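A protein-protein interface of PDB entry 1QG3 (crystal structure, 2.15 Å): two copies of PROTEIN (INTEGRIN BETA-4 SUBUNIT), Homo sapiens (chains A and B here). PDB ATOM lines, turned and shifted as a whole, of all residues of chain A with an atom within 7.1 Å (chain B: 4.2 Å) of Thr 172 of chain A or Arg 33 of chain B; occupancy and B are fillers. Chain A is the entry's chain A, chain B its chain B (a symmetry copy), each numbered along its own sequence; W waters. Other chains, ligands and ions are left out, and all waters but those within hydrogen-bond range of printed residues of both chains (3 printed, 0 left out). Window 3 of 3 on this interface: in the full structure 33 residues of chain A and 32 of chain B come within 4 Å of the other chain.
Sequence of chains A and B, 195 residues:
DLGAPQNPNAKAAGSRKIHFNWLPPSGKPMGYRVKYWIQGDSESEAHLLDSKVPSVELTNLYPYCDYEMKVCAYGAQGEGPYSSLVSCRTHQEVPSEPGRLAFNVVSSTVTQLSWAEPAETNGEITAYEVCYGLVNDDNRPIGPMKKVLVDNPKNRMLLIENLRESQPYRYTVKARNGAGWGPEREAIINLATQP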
ATOM      1  N   PRO A  98     -16.035  15.679 -21.148  1.00  0.00           N
ATOM      2  CA  PRO A  98     -16.334  15.352 -22.544  1.00  0.00           C
ATOM      3  C   PRO A  98     -15.735  16.498 -23.359  1.00  0.00           C
ATOM      4  O   PRO A  98     -15.253  17.467 -22.782  1.00  0.00           O
ATOM      5  CB  PRO A  98     -17.858  15.369 -22.577  1.00  0.00           C
ATOM      6  CG  PRO A  98     -18.221  14.881 -21.209  1.00  0.00           C
ATOM      7  CD  PRO A  98     -17.259  15.651 -20.325  1.00  0.00           C
ATOM      8  N   LEU A 101     -18.670  21.506 -25.915  1.00  0.00           N
ATOM      9  CA  LEU A 101     -20.015  21.395 -26.469  1.00  0.00           C
ATOM     10  C   LEU A 101     -20.251  22.175 -27.765  1.00  0.00           C
ATOM     11  O   LEU A 101     -19.814  23.316 -27.907  1.00  0.00           O
ATOM     12  CB  LEU A 101     -21.037  21.813 -25.407  1.00  0.00           C
ATOM     13  CG  LEU A 101     -20.845  21.160 -24.030  1.00  0.00           C
ATOM     14  CD1 LEU A 101     -22.058  21.474 -23.159  1.00  0.00           C
ATOM     15  CD2 LEU A 101     -20.661  19.653 -24.165  1.00  0.00           C
ATOM     16  N   PHE A 103     -23.277  23.365 -30.619  1.00  0.00           N
ATOM     17  CA  PHE A 103     -24.718  23.561 -30.751  1.00  0.00           C
ATOM     18  C   PHE A 103     -25.183  23.915 -32.157  1.00  0.00           C
ATOM     19  O   PHE A 103     -24.595  24.765 -32.828  1.00  0.00           O
ATOM     20  CB  PHE A 103     -25.203  24.669 -29.803  1.00  0.00           C
ATOM     21  CG  PHE A 103     -24.958  24.385 -28.347  1.00  0.00           C
ATOM     22  CD1 PHE A 103     -23.703  24.598 -27.783  1.00  0.00           C
ATOM     23  CD2 PHE A 103     -25.985  23.905 -27.537  1.00  0.00           C
ATOM     24  CE1 PHE A 103     -23.474  24.336 -26.431  1.00  0.00           C
ATOM     25  CE2 PHE A 103     -25.766  23.638 -26.181  1.00  0.00           C
ATOM     26  CZ  PHE A 103     -24.510  23.855 -25.629  1.00  0.00           C
ATOM     27  N   LEU A 113     -27.425  19.293 -29.362  1.00  0.00           N
ATOM     28  CA  LEU A 113     -26.187  19.386 -28.595  1.00  0.00           C
ATOM     29  C   LEU A 113     -25.321  18.176 -28.885  1.00  0.00           C
ATOM     30  O   LEU A 113     -25.793  17.042 -28.808  1.00  0.00           O
ATOM     31  CB  LEU A 113     -26.490  19.436 -27.095  1.00  0.00           C
ATOM     32  CG  LEU A 113     -25.298  19.168 -26.170  1.00  0.00           C
ATOM     33  CD1 LEU A 113     -24.387  20.370 -26.167  1.00  0.00           C
ATOM     34  CD2 LEU A 113     -25.781  18.876 -24.760  1.00  0.00           C
ATOM     35  N   GLU A 129     -24.474  12.047 -19.163  1.00  0.00           N
ATOM     36  CA  GLU A 129     -25.655  12.662 -18.578  1.00  0.00           C
ATOM     37  C   GLU A 129     -25.648  14.116 -19.020  1.00  0.00           C
ATOM     38  O   GLU A 129     -24.647  14.810 -18.847  1.00  0.00           O
ATOM     39  CB  GLU A 129     -25.655  12.606 -17.047  1.00  0.00           C
ATOM     40  CG  GLU A 129     -26.999  13.061 -16.461  1.00  0.00           C
ATOM     41  CD  GLU A 129     -26.987  13.206 -14.951  1.00  0.00           C
ATOM     42  OE1 GLU A 129     -26.050  13.826 -14.405  1.00  0.00           O
ATOM     43  OE2 GLU A 129     -27.926  12.707 -14.305  1.00  0.00           O
ATOM     44  N   VAL A 130     -26.747  14.564 -19.620  1.00  0.00           N
ATOM     45  CA  VAL A 130     -26.853  15.948 -20.062  1.00  0.00           C
ATOM     46  C   VAL A 130     -27.733  16.687 -19.056  1.00  0.00           C
ATOM     47  O   VAL A 130     -28.769  16.170 -18.639  1.00  0.00           O
ATOM     48  CB  VAL A 130     -27.491  16.046 -21.478  1.00  0.00           C
ATOM     49  CG1 VAL A 130     -27.564  17.512 -21.917  1.00  0.00           C
ATOM     50  CG2 VAL A 130     -26.675  15.219 -22.483  1.00  0.00           C
ATOM     51  N   CYS A 131     -27.308  17.879 -18.650  1.00  0.00           N
ATOM     52  CA  CYS A 131     -28.069  18.685 -17.692  1.00  0.00           C
ATOM     53  C   CYS A 131     -28.140  20.115 -18.224  1.00  0.00           C
ATOM     54  O   CYS A 131     -27.168  20.618 -18.777  1.00  0.00           O
ATOM     55  CB  CYS A 131     -27.379  18.705 -16.325  1.00  0.00           C
ATOM     56  SG  CYS A 131     -27.003  17.088 -15.575  1.00  0.00           S
ATOM     57  N   TYR A 132     -29.283  20.773 -18.052  1.00  0.00           N
ATOM     58  CA  TYR A 132     -29.425  22.146 -18.526  1.00  0.00           C
ATOM     59  C   TYR A 132     -30.566  22.873 -17.832  1.00  0.00           C
ATOM     60  O   TYR A 132     -31.533  22.246 -17.381  1.00  0.00           O
ATOM     61  CB  TYR A 132     -29.656  22.171 -20.041  1.00  0.00           C
ATOM     62  CG  TYR A 132     -30.930  21.483 -20.490  1.00  0.00           C
ATOM     63  CD1 TYR A 132     -30.973  20.098 -20.681  1.00  0.00           C
ATOM     64  CD2 TYR A 132     -32.098  22.215 -20.713  1.00  0.00           C
ATOM     65  CE1 TYR A 132     -32.149  19.459 -21.086  1.00  0.00           C
ATOM     66  CE2 TYR A 132     -33.281  21.590 -21.115  1.00  0.00           C
ATOM     67  CZ  TYR A 132     -33.304  20.215 -21.298  1.00  0.00           C
ATOM     68  OH  TYR A 132     -34.477  19.598 -21.682  1.00  0.00           O
ATOM     69  N   GLY A 133     -30.443  24.199 -17.752  1.00  0.00           N
ATOM     70  CA  GLY A 133     -31.463  25.021 -17.122  1.00  0.00           C
ATOM     71  C   GLY A 133     -31.219  26.504 -17.370  1.00  0.00           C
ATOM     72  O   GLY A 133     -30.148  26.884 -17.842  1.00  0.00           O
ATOM     73  N   ASN A 139     -24.959  34.488 -15.833  1.00  0.00           N
ATOM     74  CA  ASN A 139     -24.782  33.066 -16.110  1.00  0.00           C
ATOM     75  C   ASN A 139     -25.080  32.197 -14.897  1.00  0.00           C
ATOM     76  O   ASN A 139     -24.650  31.051 -14.836  1.00  0.00           O
ATOM     77  CB  ASN A 139     -23.358  32.777 -16.591  1.00  0.00           C
ATOM     78  CG  ASN A 139     -22.956  33.630 -17.776  1.00  0.00           C
ATOM     79  OD1 ASN A 139     -23.711  33.783 -18.737  1.00  0.00           O
ATOM     80  ND2 ASN A 139     -21.749  34.181 -17.719  1.00  0.00           N
ATOM     81  N   PRO A 141     -27.552  29.961 -12.584  1.00  0.00           N
ATOM     82  CA  PRO A 141     -28.808  29.205 -12.645  1.00  0.00           C
ATOM     83  C   PRO A 141     -29.911  29.910 -11.857  1.00  0.00           C
ATOM     84  O   PRO A 141     -29.687  30.344 -10.729  1.00  0.00           O
ATOM     85  CB  PRO A 141     -28.430  27.862 -12.029  1.00  0.00           C
ATOM     86  CG  PRO A 141     -27.008  27.690 -12.470  1.00  0.00           C
ATOM     87  CD  PRO A 141     -26.421  29.077 -12.243  1.00  0.00           C
ATOM     88  N   MET A 145     -32.797  22.207 -12.798  1.00  0.00           N
ATOM     89  CA  MET A 145     -32.096  21.656 -13.951  1.00  0.00           C
ATOM     90  C   MET A 145     -32.926  20.534 -14.556  1.00  0.00           C
ATOM     91  O   MET A 145     -33.724  19.898 -13.870  1.00  0.00           O
ATOM     92  CB  MET A 145     -30.740  21.065 -13.551  1.00  0.00           C
ATOM     93  CG  MET A 145     -29.627  22.051 -13.261  1.00  0.00           C
ATOM     94  SD  MET A 145     -28.030  21.177 -13.085  1.00  0.00           S
ATOM     95  CE  MET A 145     -28.149  20.598 -11.395  1.00  0.00           C
ATOM     96  N   LYS A 146     -32.744  20.306 -15.849  1.00  0.00           N
ATOM     97  CA  LYS A 146     -33.416  19.207 -16.524  1.00  0.00           C
ATOM     98  C   LYS A 146     -32.275  18.246 -16.808  1.00  0.00           C
ATOM     99  O   LYS A 146     -31.207  18.669 -17.247  1.00  0.00           O
ATOM    100  CB  LYS A 146     -34.071  19.668 -17.830  1.00  0.00           C
ATOM    101  CG  LYS A 146     -35.495  20.180 -17.640  1.00  0.00           C
ATOM    102  CD  LYS A 146     -36.093  20.671 -18.941  1.00  0.00           C
ATOM    103  CE  LYS A 146     -37.547  21.055 -18.748  1.00  0.00           C
ATOM    104  NZ  LYS A 146     -37.698  22.077 -17.673  1.00  0.00           N
ATOM    105  N   LYS A 147     -32.489  16.962 -16.540  1.00  0.00           N
ATOM    106  CA  LYS A 147     -31.443  15.967 -16.751  1.00  0.00           C
ATOM    107  C   LYS A 147     -31.871  14.827 -17.656  1.00  0.00           C
ATOM    108  O   LYS A 147     -32.981  14.306 -17.540  1.00  0.00           O
ATOM    109  CB  LYS A 147     -30.966  15.432 -15.396  1.00  0.00           C
ATOM    110  CG  LYS A 147     -30.284  16.517 -14.556  1.00  0.00           C
ATOM    111  CD  LYS A 147     -29.796  16.014 -13.197  1.00  0.00           C
ATOM    112  CE  LYS A 147     -29.003  17.107 -12.474  1.00  0.00           C
ATOM    113  NZ  LYS A 147     -28.543  16.694 -11.114  1.00  0.00           N
ATOM    114  N   ARG A 170     -27.726  27.136 -19.329  1.00  0.00           N
ATOM    115  CA  ARG A 170     -26.420  26.559 -19.048  1.00  0.00           C
ATOM    116  C   ARG A 170     -26.539  25.070 -19.347  1.00  0.00           C
ATOM    117  O   ARG A 170     -27.440  24.413 -18.827  1.00  0.00           O
ATOM    118  CB  ARG A 170     -26.016  26.724 -17.587  1.00  0.00           C
ATOM    119  CG  ARG A 170     -24.647  26.106 -17.312  1.00  0.00           C
ATOM    120  CD  ARG A 170     -24.194  26.325 -15.884  1.00  0.00           C
ATOM    121  NE  ARG A 170     -24.788  25.346 -14.993  1.00  0.00           N
ATOM    122  CZ  ARG A 170     -24.668  25.377 -13.672  1.00  0.00           C
ATOM    123  NH1 ARG A 170     -23.970  26.345 -13.090  1.00  0.00           N
ATOM    124  NH2 ARG A 170     -25.251  24.442 -12.936  1.00  0.00           N
ATOM    125  N   TYR A 171     -25.648  24.545 -20.186  1.00  0.00           N
ATOM    126  CA  TYR A 171     -25.662  23.128 -20.538  1.00  0.00           C
ATOM    127  C   TYR A 171     -24.398  22.442 -20.033  1.00  0.00           C
ATOM    128  O   TYR A 171     -23.318  23.027 -20.090  1.00  0.00           O
ATOM    129  CB  TYR A 171     -25.700  22.933 -22.057  1.00  0.00           C
ATOM    130  CG  TYR A 171     -26.897  23.502 -22.776  1.00  0.00           C
ATOM    131  CD1 TYR A 171     -26.926  24.840 -23.172  1.00  0.00           C
ATOM    132  CD2 TYR A 171     -27.994  22.696 -23.083  1.00  0.00           C
ATOM    133  CE1 TYR A 171     -28.017  25.363 -23.858  1.00  0.00           C
ATOM    134  CE2 TYR A 171     -29.092  23.210 -23.770  1.00  0.00           C
ATOM    135  CZ  TYR A 171     -29.095  24.543 -24.153  1.00  0.00           C
ATOM    136  OH  TYR A 171     -30.173  25.053 -24.826  1.00  0.00           O
ATOM    137  N   THR A 172     -24.527  21.206 -19.549  1.00  0.00           N
ATOM    138  CA  THR A 172     -23.360  20.447 -19.093  1.00  0.00           C
ATOM    139  C   THR A 172     -23.479  18.978 -19.495  1.00  0.00           C
ATOM    140  O   THR A 172     -24.571  18.428 -19.582  1.00  0.00           O
ATOM    141  CB  THR A 172     -23.172  20.479 -17.558  1.00  0.00           C
ATOM    142  OG1 THR A 172     -24.259  19.793 -16.934  1.00  0.00           O
ATOM    143  CG2 THR A 172     -23.087  21.921 -17.034  1.00  0.00           C
ATOM    144  N   VAL A 173     -22.339  18.350 -19.749  1.00  0.00           N
ATOM    145  CA  VAL A 173     -22.306  16.939 -20.108  1.00  0.00           C
ATOM    146  C   VAL A 173     -21.190  16.317 -19.284  1.00  0.00           C
ATOM    147  O   VAL A 173     -20.096  16.880 -19.208  1.00  0.00           O
ATOM    148  CB  VAL A 173     -21.979  16.718 -21.604  1.00  0.00           C
ATOM    149  CG1 VAL A 173     -22.072  15.226 -21.934  1.00  0.00           C
ATOM    150  CG2 VAL A 173     -22.921  17.518 -22.476  1.00  0.00           C
ATOM    151  N   LYS A 174     -21.485  15.177 -18.659  1.00  0.00           N
ATOM    152  CA  LYS A 174     -20.524  14.438 -17.844  1.00  0.00           C
ATOM    153  C   LYS A 174     -20.596  12.961 -18.276  1.00  0.00           C
ATOM    154  O   LYS A 174     -21.654  12.491 -18.711  1.00  0.00           O
ATOM    155  CB  LYS A 174     -20.869  14.591 -16.360  1.00  0.00           C
ATOM    156  CG  LYS A 174     -22.251  14.082 -15.988  1.00  0.00           C
ATOM    157  CD  LYS A 174     -22.568  14.383 -14.532  1.00  0.00           C
ATOM    158  CE  LYS A 174     -22.865  15.860 -14.322  1.00  0.00           C
ATOM    159  NZ  LYS A 174     -24.082  16.307 -15.068  1.00  0.00           N
ATOM    160  N   GLU A 184     -17.802  17.737 -15.385  1.00  0.00           N
ATOM    161  CA  GLU A 184     -18.656  18.204 -16.481  1.00  0.00           C
ATOM    162  C   GLU A 184     -18.013  19.220 -17.425  1.00  0.00           C
ATOM    163  O   GLU A 184     -17.165  20.013 -17.016  1.00  0.00           O
ATOM    164  CB  GLU A 184     -19.933  18.865 -15.938  1.00  0.00           C
ATOM    165  CG  GLU A 184     -20.430  18.343 -14.612  1.00  0.00           C
ATOM    166  CD  GLU A 184     -21.537  19.199 -14.041  1.00  0.00           C
ATOM    167  OE1 GLU A 184     -21.409  20.442 -14.074  1.00  0.00           O
ATOM    168  OE2 GLU A 184     -22.531  18.632 -13.551  1.00  0.00           O
ATOM    169  N   ARG A 185     -18.450  19.185 -18.683  1.00  0.00           N
ATOM    170  CA  ARG A 185     -18.027  20.130 -19.722  1.00  0.00           C
ATOM    171  C   ARG A 185     -19.213  21.095 -19.755  1.00  0.00           C
ATOM    172  O   ARG A 185     -20.361  20.653 -19.790  1.00  0.00           O
ATOM    173  CB  ARG A 185     -17.909  19.442 -21.079  1.00  0.00           C
ATOM    174  CG  ARG A 185     -17.204  20.285 -22.101  1.00  0.00           C
ATOM    175  CD  ARG A 185     -15.738  20.340 -21.752  1.00  0.00           C
ATOM    176  NE  ARG A 185     -14.969  21.161 -22.669  1.00  0.00           N
ATOM    177  CZ  ARG A 185     -13.647  21.091 -22.779  1.00  0.00           C
ATOM    178  NH1 ARG A 185     -12.967  20.235 -22.031  1.00  0.00           N
ATOM    179  NH2 ARG A 185     -13.010  21.870 -23.640  1.00  0.00           N
ATOM    180  N   GLU A 186     -18.948  22.395 -19.776  1.00  0.00           N
ATOM    181  CA  GLU A 186     -20.019  23.381 -19.713  1.00  0.00           C
ATOM    182  C   GLU A 186     -20.100  24.395 -20.854  1.00  0.00           C
ATOM    183  O   GLU A 186     -19.118  24.655 -21.547  1.00  0.00           O
ATOM    184  CB  GLU A 186     -19.870  24.118 -18.380  1.00  0.00           C
ATOM    185  CG  GLU A 186     -20.981  25.060 -17.995  1.00  0.00           C
ATOM    186  CD  GLU A 186     -20.618  25.847 -16.749  1.00  0.00           C
ATOM    187  OE1 GLU A 186     -19.697  26.690 -16.814  1.00  0.00           O
ATOM    188  OE2 GLU A 186     -21.243  25.613 -15.701  1.00  0.00           O
ATOM    189  N   ALA A 187     -21.291  24.968 -21.039  1.00  0.00           N
ATOM    190  CA  ALA A 187     -21.520  25.989 -22.059  1.00  0.00           C
ATOM    191  C   ALA A 187     -22.788  26.790 -21.769  1.00  0.00           C
ATOM    192  O   ALA A 187     -23.817  26.229 -21.384  1.00  0.00           O
ATOM    193  CB  ALA A 187     -21.610  25.356 -23.437  1.00  0.00           C
ATOM    194  N   TYR B  32     -25.209  19.674  -5.210  1.00  0.00           N
ATOM    195  CA  TYR B  32     -24.103  20.610  -5.083  1.00  0.00           C
ATOM    196  C   TYR B  32     -23.188  20.611  -6.291  1.00  0.00           C
ATOM    197  O   TYR B  32     -22.975  19.577  -6.924  1.00  0.00           O
ATOM    198  CB  TYR B  32     -23.258  20.238  -3.865  1.00  0.00           C
ATOM    199  CG  TYR B  32     -24.029  20.158  -2.574  1.00  0.00           C
ATOM    200  CD1 TYR B  32     -24.332  21.312  -1.844  1.00  0.00           C
ATOM    201  CD2 TYR B  32     -24.483  18.932  -2.090  1.00  0.00           C
ATOM    202  CE1 TYR B  32     -25.068  21.245  -0.669  1.00  0.00           C
ATOM    203  CE2 TYR B  32     -25.223  18.857  -0.911  1.00  0.00           C
ATOM    204  CZ  TYR B  32     -25.512  20.018  -0.209  1.00  0.00           C
ATOM    205  OH  TYR B  32     -26.259  19.952   0.943  1.00  0.00           O
ATOM    206  N   ARG B  33     -22.649  21.781  -6.608  1.00  0.00           N
ATOM    207  CA  ARG B  33     -21.690  21.894  -7.695  1.00  0.00           C
ATOM    208  C   ARG B  33     -20.362  22.278  -7.054  1.00  0.00           C
ATOM    209  O   ARG B  33     -20.275  23.283  -6.339  1.00  0.00           O
ATOM    210  CB  ARG B  33     -22.083  22.974  -8.700  1.00  0.00           C
ATOM    211  CG  ARG B  33     -20.862  23.561  -9.395  1.00  0.00           C
ATOM    212  CD  ARG B  33     -21.213  24.504 -10.525  1.00  0.00           C
ATOM    213  NE  ARG B  33     -21.428  23.787 -11.778  1.00  0.00           N
ATOM    214  CZ  ARG B  33     -21.295  24.346 -12.974  1.00  0.00           C
ATOM    215  NH1 ARG B  33     -20.949  25.625 -13.067  1.00  0.00           N
ATOM    216  NH2 ARG B  33     -21.492  23.628 -14.071  1.00  0.00           N
ATOM    217  N   VAL B  34     -19.340  21.464  -7.290  1.00  0.00           N
ATOM    218  CA  VAL B  34     -18.012  21.723  -6.751  1.00  0.00           C
ATOM    219  C   VAL B  34     -17.112  22.229  -7.871  1.00  0.00           C
ATOM    220  O   VAL B  34     -17.105  21.679  -8.977  1.00  0.00           O
ATOM    221  CB  VAL B  34     -17.368  20.453  -6.167  1.00  0.00           C
ATOM    222  CG1 VAL B  34     -15.914  20.721  -5.848  1.00  0.00           C
ATOM    223  CG2 VAL B  34     -18.103  20.011  -4.917  1.00  0.00           C
ATOM    224  N   LYS B  35     -16.359  23.284  -7.585  1.00  0.00           N
ATOM    225  CA  LYS B  35     -15.441  23.852  -8.559  1.00  0.00           C
ATOM    226  C   LYS B  35     -14.053  23.739  -7.952  1.00  0.00           C
ATOM    227  O   LYS B  35     -13.861  24.087  -6.787  1.00  0.00           O
ATOM    228  CB  LYS B  35     -15.790  25.323  -8.811  1.00  0.00           C
ATOM    229  CG  LYS B  35     -15.040  25.956  -9.973  1.00  0.00           C
ATOM    230  CD  LYS B  35     -15.557  27.364 -10.269  1.00  0.00           C
ATOM    231  CE  LYS B  35     -14.818  27.987 -11.456  1.00  0.00           C
ATOM    232  NZ  LYS B  35     -15.191  29.418 -11.679  1.00  0.00           N
ATOM    233  N   LEU B  48     -15.306  20.965 -12.958  1.00  0.00           N
ATOM    234  CA  LEU B  48     -16.630  20.996 -12.352  1.00  0.00           C
ATOM    235  C   LEU B  48     -17.232  19.631 -12.039  1.00  0.00           C
ATOM    236  O   LEU B  48     -17.369  18.783 -12.919  1.00  0.00           O
ATOM    237  CB  LEU B  48     -17.580  21.751 -13.288  1.00  0.00           C
ATOM    238  CG  LEU B  48     -17.109  23.133 -13.752  1.00  0.00           C
ATOM    239  CD1 LEU B  48     -17.921  23.582 -14.961  1.00  0.00           C
ATOM    240  CD2 LEU B  48     -17.231  24.120 -12.611  1.00  0.00           C
ATOM    241  N   LEU B  49     -17.610  19.437 -10.783  1.00  0.00           N
ATOM    242  CA  LEU B  49     -18.226  18.191 -10.350  1.00  0.00           C
ATOM    243  C   LEU B  49     -19.578  18.483  -9.720  1.00  0.00           C
ATOM    244  O   LEU B  49     -19.782  19.541  -9.122  1.00  0.00           O
ATOM    245  CB  LEU B  49     -17.348  17.476  -9.317  1.00  0.00           C
ATOM    246  CG  LEU B  49     -16.156  16.658  -9.809  1.00  0.00           C
ATOM    247  CD1 LEU B  49     -15.333  16.212  -8.607  1.00  0.00           C
ATOM    248  CD2 LEU B  49     -16.647  15.445 -10.606  1.00  0.00           C
ATOM    249  N   VAL B  71     -17.623  25.213  -3.043  1.00  0.00           N
ATOM    250  CA  VAL B  71     -18.843  24.511  -3.406  1.00  0.00           C
ATOM    251  C   VAL B  71     -20.107  25.339  -3.186  1.00  0.00           C
ATOM    252  O   VAL B  71     -20.144  26.207  -2.313  1.00  0.00           O
ATOM    253  CB  VAL B  71     -18.968  23.204  -2.593  1.00  0.00           C
ATOM    254  CG1 VAL B  71     -18.920  23.516  -1.107  1.00  0.00           C
ATOM    255  CG2 VAL B  71     -20.261  22.467  -2.946  1.00  0.00           C
ATOM    256  N   CYS B  72     -21.130  25.071  -3.996  1.00  0.00           N
ATOM    257  CA  CYS B  72     -22.413  25.760  -3.867  1.00  0.00           C
ATOM    258  C   CYS B  72     -23.525  24.723  -3.969  1.00  0.00           C
ATOM    259  O   CYS B  72     -23.306  23.604  -4.440  1.00  0.00           O
ATOM    260  CB  CYS B  72     -22.598  26.816  -4.960  1.00  0.00           C
ATOM    261  SG  CYS B  72     -22.880  26.170  -6.628  1.00  0.00           S
ATOM    262  N   TYR B  74     -27.630  23.873  -5.165  1.00  0.00           N
ATOM    263  CA  TYR B  74     -28.590  24.307  -6.162  1.00  0.00           C
ATOM    264  C   TYR B  74     -29.962  23.760  -5.786  1.00  0.00           C
ATOM    265  O   TYR B  74     -30.071  22.666  -5.219  1.00  0.00           O
ATOM    266  CB  TYR B  74     -28.160  23.868  -7.574  1.00  0.00           C
ATOM    267  CG  TYR B  74     -27.897  22.391  -7.762  1.00  0.00           C
ATOM    268  CD1 TYR B  74     -28.948  21.475  -7.829  1.00  0.00           C
ATOM    269  CD2 TYR B  74     -26.591  21.911  -7.894  1.00  0.00           C
ATOM    270  CE1 TYR B  74     -28.708  20.113  -8.025  1.00  0.00           C
ATOM    271  CE2 TYR B  74     -26.337  20.555  -8.089  1.00  0.00           C
ATOM    272  CZ  TYR B  74     -27.400  19.662  -8.154  1.00  0.00           C
ATOM    273  OH  TYR B  74     -27.157  18.322  -8.340  1.00  0.00           O
ATOM    274  N   GLU B  79     -28.995  28.194  -8.328  1.00  0.00           N
ATOM    275  CA  GLU B  79     -27.806  28.081  -7.489  1.00  0.00           C
ATOM    276  C   GLU B  79     -27.704  29.124  -6.388  1.00  0.00           C
ATOM    277  O   GLU B  79     -28.020  30.294  -6.588  1.00  0.00           O
ATOM    278  CB  GLU B  79     -26.533  28.182  -8.338  1.00  0.00           C
ATOM    279  CG  GLU B  79     -26.109  26.907  -9.030  1.00  0.00           C
ATOM    280  CD  GLU B  79     -24.754  27.039  -9.702  1.00  0.00           C
ATOM    281  OE1 GLU B  79     -24.093  28.092  -9.528  1.00  0.00           O
ATOM    282  OE2 GLU B  79     -24.351  26.085 -10.403  1.00  0.00           O
ATOM    283  N   TYR B  82     -21.571  30.614  -3.476  1.00  0.00           N
ATOM    284  CA  TYR B  82     -20.511  29.651  -3.193  1.00  0.00           C
ATOM    285  C   TYR B  82     -19.966  29.765  -1.776  1.00  0.00           C
ATOM    286  O   TYR B  82     -20.033  30.824  -1.143  1.00  0.00           O
ATOM    287  CB  TYR B  82     -19.340  29.827  -4.162  1.00  0.00           C
ATOM    288  CG  TYR B  82     -19.439  28.998  -5.415  1.00  0.00           C
ATOM    289  CD1 TYR B  82     -18.964  27.688  -5.439  1.00  0.00           C
ATOM    290  CD2 TYR B  82     -19.999  29.521  -6.580  1.00  0.00           C
ATOM    291  CE1 TYR B  82     -19.042  26.916  -6.597  1.00  0.00           C
ATOM    292  CE2 TYR B  82     -20.079  28.762  -7.742  1.00  0.00           C
ATOM    293  CZ  TYR B  82     -19.597  27.462  -7.742  1.00  0.00           C
ATOM    294  OH  TYR B  82     -19.670  26.709  -8.888  1.00  0.00           O
HETATM  295  O   HOH W   1     -21.276  27.381 -11.147  1.00  0.00           O
HETATM  296  O   HOH W   2     -25.551  23.981 -10.415  1.00  0.00           O
HETATM  297  O   HOH W   3     -14.895  20.551 -15.687  1.00  0.00           O
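Water W2 bridges OE2 of Glu 79 of chain B (2.4 Å) and NH2 of Arg 170 of chain A (2.6 Å).
Water W1 lies within hydrogen-bond range of the guanidinium group of Arg 33 of chain B (2.6 Å), the side-chain hydroxyl of Tyr 82 of chain B (2.9 Å), the side-chain carboxylate of Glu 79 of chain B (3.3 Å) and the guanidinium group of Arg 170 of chain A (3.5 Å).
Water W3 bridges the backbone carbonyl oxygen (O) of Glu 184 of chain A and the backbone NH (N) of Leu 48 of chain B.
Met 145 of chain A touches Tyr 74 of chain B.
Lys 147 of chain A touches Tyr 74 of chain B (NZ to OH, 3.5 Å).
NH2 of Arg 33 of chain B touches CG2 of Thr 172 of chain A, 3.8 Å away.
CD of Glu 186 of chain A touches CD1 of Leu 48 of chain B, 3.9 Å away.
No position is printed for both chains.
Of the 10 pairs that touch across the chains among the printed residues, none has its exchanged pair printed and touching as well.
OE1 of Glu 184 of chain A lies within salt-bridge range of NH2 of Arg 33 of chain B (3.2 Å).
OE2 of Glu 186 of chain A lies within salt-bridge range of NH2 of Arg 33 of chain B, at 2.6 Å.
The guanidinium group (NH1) of Arg 170 of chain A is in salt-bridge range of the side-chain carboxylate (OE2) of Glu 79 of chain B, 2.7 Å away.
NH1 of Arg 170 of chain A lies close to NH1 of Arg 33 of chain B, at 3.1 Å.
The backbone carbonyl oxygen of Leu 48 of chain B is in hydrogen-bond range of the backbone NH of Glu 184 of chain A.
The backbone carbonyl oxygen (O) of Pro 141 of chain A is in hydrogen-bond range of the backbone NH (N) of Glu 79 of chain B (3.3 Å).
Of the printed residues of chain B, Thr 172 of chain A touches Arg 33.
Arg 33 of chain B touches four residues of chain A.
Printed residues of chain A within 4 Å of Glu 79 of chain B: Pro 141 and Arg 170.
Of the printed residues of chain B, Glu 184 of chain A touches Arg 33 and Leu 48.
Of the printed residues of chain B, Met 145 of chain A touches Tyr 74.
Printed residues of chain B within 4 Å of Glu 186 of chain A: Arg 33 (2.6 Å) and Leu 48 (3.9 Å).
Pro 98 of chain A touches none of the printed residues of chain B.
The nearest printed residue of chain B that does not touch Glu 186 of chain A is Glu 79 of chain B (6.2 Å).
The side-chain amino group (NZ) of Lys 174 of chain A lies within salt-bridge range of the side-chain carboxylate (OE2) of Glu 184 of chain A (3.2 Å).
The side-chain carboxylate (OE2) of Glu 186 of chain A lies within salt-bridge range of the guanidinium group (NE) of Arg 170 of chain A (3.6 Å).
O of Cys 131 of chain A lies within hydrogen-bond range of N of Thr 172 of chain A, at 2.8 Å.
N of Arg 170 of chain A lies within hydrogen-bond range of O of Gly 133 of chain A.
Of the 23 printed residues of chain A, 7 touch a printed residue of chain B.
Printed residues of chain A that touch a printed residue of chain B: Pro 141, Met 145, Lys 147, Arg 170, Thr 172, Glu 184 and Glu 186.
Printed residues of chain B that touch a printed residue of chain A: Arg 33, Leu 48, Tyr 74 and Glu 79.
Hydrophobic or aromatic side chains of chain B within 4 Å of the printed part of chain A: Leu 48 and Tyr 74.
Among the printed residues, 10 pairs touch across the chains.
Among the printed residues, Asp or Glu carboxylates within 4 Å of a Lys or Arg side-chain nitrogen of the other chain: Arg 170 of chain A with Glu 79 of chain B (2.7 Å), Glu 184 of chain A with Arg 33 of chain B (3.2 Å) and Glu 186 of chain A with Arg 33 of chain B (2.6 Å).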
